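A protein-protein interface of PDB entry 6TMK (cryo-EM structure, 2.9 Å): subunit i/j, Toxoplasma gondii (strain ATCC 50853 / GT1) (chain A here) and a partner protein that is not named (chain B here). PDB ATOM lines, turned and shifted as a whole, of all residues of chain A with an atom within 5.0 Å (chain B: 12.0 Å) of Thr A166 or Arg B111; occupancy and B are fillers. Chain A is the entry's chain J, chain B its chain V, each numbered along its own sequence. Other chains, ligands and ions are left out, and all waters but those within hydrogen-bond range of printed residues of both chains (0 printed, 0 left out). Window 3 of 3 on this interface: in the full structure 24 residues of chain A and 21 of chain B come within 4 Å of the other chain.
Among the printed residues, merely in contact across the chains: Arg A155 with Arg B111 (3.8 Å), Thr A166 with Pro B110 (3.998 Å), Asn A168 with Pro B110 (3.1 Å), Glu A169 with Val B109 (3.8 Å) and Glu A169 with Pro B110 (3.96 Å).
The backbone carbonyl oxygen (O) of Arg A155 lies within hydrogen-bond range of the backbone NH (N) of Leu A161.
NH1 of Arg A155 lies close to O of Pro A164.
The side-chain carboxylate (OE2) of Glu A169 is in salt-bridge range of the guanidinium group (NH2) of Arg A155.
The backbone NH (N) of Thr A166 lies within hydrogen-bond range of the side-chain carboxylate (OE1) of Glu A169.
O of Pro A164 lies within hydrogen-bond range of NH2 of Arg B111 (2.7 Å).
The side-chain hydroxyl (OG1) of Thr A166 sits at hydrogen-bond distance from the chain-end carboxylate (OXT) of Arg B111 (2.8 Å).
The guanidinium group of Arg B111 is in salt-bridge range of the side-chain carboxylate of Glu A169, at 3.3 Å.
Of the 5 printed residues of chain B, 3 touch a printed residue of chain A.
Printed residues of chain B that touch a printed residue of chain A: Val B109, Pro B110 and Arg B111.
Hydrophobic or aromatic side chains of chain B that line the printed part of chain A: Val B109.
Among the printed residues, 8 pairs touch across the chains.
Among the printed residues, Asp or Glu carboxylates within 4 Å of a Lys or Arg side-chain nitrogen of the other chain: Glu A169 with Arg B111 (3.3 Å).
Of the printed residues of chain B, Thr A166 touches Pro B110 and Arg B111.
Arg B111 touches just these residues of chain A: Arg A155, Pro A164, Thr A166 and Glu A169.
Pro A164 touches just one residue of chain B: Arg B111.
No residue of chain B comes within 4 Å of Phe A165.
No residue of chain B comes within 4 Å of Leu A167.
Of the printed residues of chain B, Glu A169 touches Val B109, Pro B110 and Arg B111.
No residue of chain B comes within 4 Å of Met A170.
Printed residues of chain A within 4 Å of Val B109: Glu A169 (3.8 Å).
Of the printed residues of chain A, Pro B110 touches Thr A166, Asn A168 and Glu A169.
Of the printed residues of chain B, Arg A155 touches Arg B111.
The nearest printed residue of chain B that does not touch Thr A166 is Val B109 (6.6 Å).
The nearest printed residue of chain A that does not touch Val B109 is Asn A168 (4.4 Å).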
ATOM      1  N   ARG A 155       2.156  16.328   8.493  1.00  0.00           N
ATOM      2  CA  ARG A 155       0.885  15.742   8.096  1.00  0.00           C
ATOM      3  C   ARG A 155       0.801  15.434   6.606  1.00  0.00           C
ATOM      4  O   ARG A 155       0.130  14.471   6.226  1.00  0.00           O
ATOM      5  CB  ARG A 155      -0.261  16.665   8.490  1.00  0.00           C
ATOM      6  CG  ARG A 155      -0.493  16.731   9.964  1.00  0.00           C
ATOM      7  CD  ARG A 155      -1.646  17.615  10.313  1.00  0.00           C
ATOM      8  NE  ARG A 155      -1.785  17.782  11.752  1.00  0.00           N
ATOM      9  CZ  ARG A 155      -2.275  18.867  12.335  1.00  0.00           C
ATOM     10  NH1 ARG A 155      -2.687  19.890  11.614  1.00  0.00           N
ATOM     11  NH2 ARG A 155      -2.352  18.929  13.647  1.00  0.00           N
ATOM     12  N   LEU A 161      -1.758  13.071   4.230  1.00  0.00           N
ATOM     13  CA  LEU A 161      -2.950  13.901   4.211  1.00  0.00           C
ATOM     14  C   LEU A 161      -2.784  15.000   3.174  1.00  0.00           C
ATOM     15  O   LEU A 161      -1.864  15.816   3.269  1.00  0.00           O
ATOM     16  CB  LEU A 161      -3.197  14.508   5.587  1.00  0.00           C
ATOM     17  CG  LEU A 161      -3.242  13.536   6.762  1.00  0.00           C
ATOM     18  CD1 LEU A 161      -3.510  14.293   8.026  1.00  0.00           C
ATOM     19  CD2 LEU A 161      -4.295  12.483   6.551  1.00  0.00           C
ATOM     20  N   HIS A 163      -4.962  17.379   2.734  1.00  0.00           N
ATOM     21  CA  HIS A 163      -5.579  18.575   3.298  1.00  0.00           C
ATOM     22  C   HIS A 163      -5.291  18.603   4.790  1.00  0.00           C
ATOM     23  O   HIS A 163      -6.157  18.283   5.615  1.00  0.00           O
ATOM     24  CB  HIS A 163      -7.072  18.602   2.990  1.00  0.00           C
ATOM     25  CG  HIS A 163      -7.377  18.392   1.545  1.00  0.00           C
ATOM     26  ND1 HIS A 163      -7.052  19.317   0.579  1.00  0.00           N
ATOM     27  CD2 HIS A 163      -7.943  17.351   0.895  1.00  0.00           C
ATOM     28  CE1 HIS A 163      -7.423  18.862  -0.602  1.00  0.00           C
ATOM     29  NE2 HIS A 163      -7.964  17.670  -0.439  1.00  0.00           N
ATOM     30  N   PRO A 164      -4.072  18.982   5.173  1.00  0.00           N
ATOM     31  CA  PRO A 164      -3.679  18.871   6.581  1.00  0.00           C
ATOM     32  C   PRO A 164      -4.324  19.908   7.476  1.00  0.00           C
ATOM     33  O   PRO A 164      -4.545  19.633   8.659  1.00  0.00           O
ATOM     34  CB  PRO A 164      -2.154  19.040   6.529  1.00  0.00           C
ATOM     35  CG  PRO A 164      -1.799  19.116   5.100  1.00  0.00           C
ATOM     36  CD  PRO A 164      -2.985  19.528   4.359  1.00  0.00           C
ATOM     37  N   PHE A 165      -4.610  21.093   6.956  1.00  0.00           N
ATOM     38  CA  PHE A 165      -5.052  22.225   7.751  1.00  0.00           C
ATOM     39  C   PHE A 165      -6.554  22.397   7.614  1.00  0.00           C
ATOM     40  O   PHE A 165      -7.080  22.470   6.499  1.00  0.00           O
ATOM     41  CB  PHE A 165      -4.335  23.504   7.320  1.00  0.00           C
ATOM     42  CG  PHE A 165      -3.012  23.718   7.983  1.00  0.00           C
ATOM     43  CD1 PHE A 165      -2.419  22.724   8.727  1.00  0.00           C
ATOM     44  CD2 PHE A 165      -2.348  24.917   7.846  1.00  0.00           C
ATOM     45  CE1 PHE A 165      -1.215  22.920   9.327  1.00  0.00           C
ATOM     46  CE2 PHE A 165      -1.132  25.114   8.445  1.00  0.00           C
ATOM     47  CZ  PHE A 165      -0.564  24.113   9.183  1.00  0.00           C
ATOM     48  N   THR A 166      -7.236  22.447   8.750  1.00  0.00           N
ATOM     49  CA  THR A 166      -8.620  22.875   8.785  1.00  0.00           C
ATOM     50  C   THR A 166      -8.688  24.398   8.764  1.00  0.00           C
ATOM     51  O   THR A 166      -7.680  25.101   8.645  1.00  0.00           O
ATOM     52  CB  THR A 166      -9.336  22.310  10.012  1.00  0.00           C
ATOM     53  OG1 THR A 166      -8.862  22.954  11.200  1.00  0.00           O
ATOM     54  CG2 THR A 166      -9.130  20.818  10.121  1.00  0.00           C
ATOM     55  N   LEU A 167      -9.906  24.913   8.883  1.00  0.00           N
ATOM     56  CA  LEU A 167     -10.114  26.351   8.822  1.00  0.00           C
ATOM     57  C   LEU A 167      -9.443  27.048  10.000  1.00  0.00           C
ATOM     58  O   LEU A 167      -8.869  28.133   9.848  1.00  0.00           O
ATOM     59  CB  LEU A 167     -11.616  26.611   8.786  1.00  0.00           C
ATOM     60  CG  LEU A 167     -12.175  27.871   8.151  1.00  0.00           C
ATOM     61  CD1 LEU A 167     -11.805  27.881   6.698  1.00  0.00           C
ATOM     62  CD2 LEU A 167     -13.676  27.876   8.303  1.00  0.00           C
ATOM     63  N   ASN A 168      -9.482  26.422  11.176  1.00  0.00           N
ATOM     64  CA  ASN A 168      -8.822  26.977  12.353  1.00  0.00           C
ATOM     65  C   ASN A 168      -7.320  27.094  12.129  1.00  0.00           C
ATOM     66  O   ASN A 168      -6.712  28.128  12.428  1.00  0.00           O
ATOM     67  CB  ASN A 168      -9.126  26.121  13.576  1.00  0.00           C
ATOM     68  CG  ASN A 168     -10.340  26.598  14.332  1.00  0.00           C
ATOM     69  OD1 ASN A 168     -10.546  27.795  14.513  1.00  0.00           O
ATOM     70  ND2 ASN A 168     -11.148  25.664  14.784  1.00  0.00           N
ATOM     71  N   GLU A 169      -6.696  26.021  11.645  1.00  0.00           N
ATOM     72  CA  GLU A 169      -5.258  26.027  11.424  1.00  0.00           C
ATOM     73  C   GLU A 169      -4.875  27.018  10.335  1.00  0.00           C
ATOM     74  O   GLU A 169      -3.808  27.637  10.401  1.00  0.00           O
ATOM     75  CB  GLU A 169      -4.793  24.623  11.063  1.00  0.00           C
ATOM     76  CG  GLU A 169      -4.944  23.599  12.153  1.00  0.00           C
ATOM     77  CD  GLU A 169      -5.217  22.212  11.622  1.00  0.00           C
ATOM     78  OE1 GLU A 169      -6.274  22.015  10.995  1.00  0.00           O
ATOM     79  OE2 GLU A 169      -4.370  21.319  11.822  1.00  0.00           O
ATOM     80  N   MET A 170      -5.734  27.186   9.334  1.00  0.00           N
ATOM     81  CA  MET A 170      -5.487  28.182   8.301  1.00  0.00           C
ATOM     82  C   MET A 170      -5.509  29.586   8.888  1.00  0.00           C
ATOM     83  O   MET A 170      -4.635  30.414   8.592  1.00  0.00           O
ATOM     84  CB  MET A 170      -6.539  28.023   7.204  1.00  0.00           C
ATOM     85  CG  MET A 170      -6.108  28.417   5.827  1.00  0.00           C
ATOM     86  SD  MET A 170      -4.687  27.513   5.220  1.00  0.00           S
ATOM     87  CE  MET A 170      -3.690  28.915   4.757  1.00  0.00           C
ATOM     88  N   ASN B 107      -2.058  25.657  24.307  1.00  0.00           N
ATOM     89  CA  ASN B 107      -2.690  24.455  23.814  1.00  0.00           C
ATOM     90  C   ASN B 107      -2.431  24.309  22.322  1.00  0.00           C
ATOM     91  O   ASN B 107      -2.164  25.289  21.628  1.00  0.00           O
ATOM     92  CB  ASN B 107      -4.186  24.490  24.079  1.00  0.00           C
ATOM     93  CG  ASN B 107      -4.515  24.720  25.523  1.00  0.00           C
ATOM     94  OD1 ASN B 107      -3.690  24.511  26.407  1.00  0.00           O
ATOM     95  ND2 ASN B 107      -5.725  25.172  25.775  1.00  0.00           N
ATOM     96  N   PRO B 108      -2.509  23.091  21.801  1.00  0.00           N
ATOM     97  CA  PRO B 108      -2.352  22.900  20.360  1.00  0.00           C
ATOM     98  C   PRO B 108      -3.446  23.600  19.574  1.00  0.00           C
ATOM     99  O   PRO B 108      -4.533  23.885  20.078  1.00  0.00           O
ATOM    100  CB  PRO B 108      -2.429  21.379  20.196  1.00  0.00           C
ATOM    101  CG  PRO B 108      -3.080  20.894  21.412  1.00  0.00           C
ATOM    102  CD  PRO B 108      -2.674  21.809  22.497  1.00  0.00           C
ATOM    103  N   VAL B 109      -3.141  23.884  18.318  1.00  0.00           N
ATOM    104  CA  VAL B 109      -4.103  24.602  17.479  1.00  0.00           C
ATOM    105  C   VAL B 109      -5.330  23.722  17.277  1.00  0.00           C
ATOM    106  O   VAL B 109      -5.185  22.536  16.933  1.00  0.00           O
ATOM    107  CB  VAL B 109      -3.474  24.978  16.141  1.00  0.00           C
ATOM    108  CG1 VAL B 109      -4.474  25.739  15.298  1.00  0.00           C
ATOM    109  CG2 VAL B 109      -2.225  25.796  16.354  1.00  0.00           C
ATOM    110  N   PRO B 110      -6.541  24.233  17.476  1.00  0.00           N
ATOM    111  CA  PRO B 110      -7.718  23.376  17.329  1.00  0.00           C
ATOM    112  C   PRO B 110      -7.916  22.950  15.887  1.00  0.00           C
ATOM    113  O   PRO B 110      -7.737  23.738  14.955  1.00  0.00           O
ATOM    114  CB  PRO B 110      -8.871  24.265  17.807  1.00  0.00           C
ATOM    115  CG  PRO B 110      -8.232  25.476  18.410  1.00  0.00           C
ATOM    116  CD  PRO B 110      -6.924  25.623  17.756  1.00  0.00           C
ATOM    117  N   ARG B 111      -8.273  21.686  15.707  1.00  0.00           N
ATOM    118  CA  ARG B 111      -8.512  21.160  14.378  1.00  0.00           C
ATOM    119  C   ARG B 111     -10.008  21.189  14.083  1.00  0.00           C
ATOM    120  O   ARG B 111     -10.827  20.939  14.965  1.00  0.00           O
ATOM    121  CB  ARG B 111      -7.964  19.741  14.236  1.00  0.00           C
ATOM    122  CG  ARG B 111      -6.463  19.649  14.110  1.00  0.00           C
ATOM    123  CD  ARG B 111      -6.106  18.447  13.276  1.00  0.00           C
ATOM    124  NE  ARG B 111      -6.331  18.700  11.860  1.00  0.00           N
ATOM    125  CZ  ARG B 111      -6.245  17.778  10.913  1.00  0.00           C
ATOM    126  NH1 ARG B 111      -5.935  16.530  11.226  1.00  0.00           N
ATOM    127  NH2 ARG B 111      -6.476  18.111   9.652  1.00  0.00           N
ATOM    128  OXT ARG B 111     -10.433  21.463  12.961  1.00  0.00           O
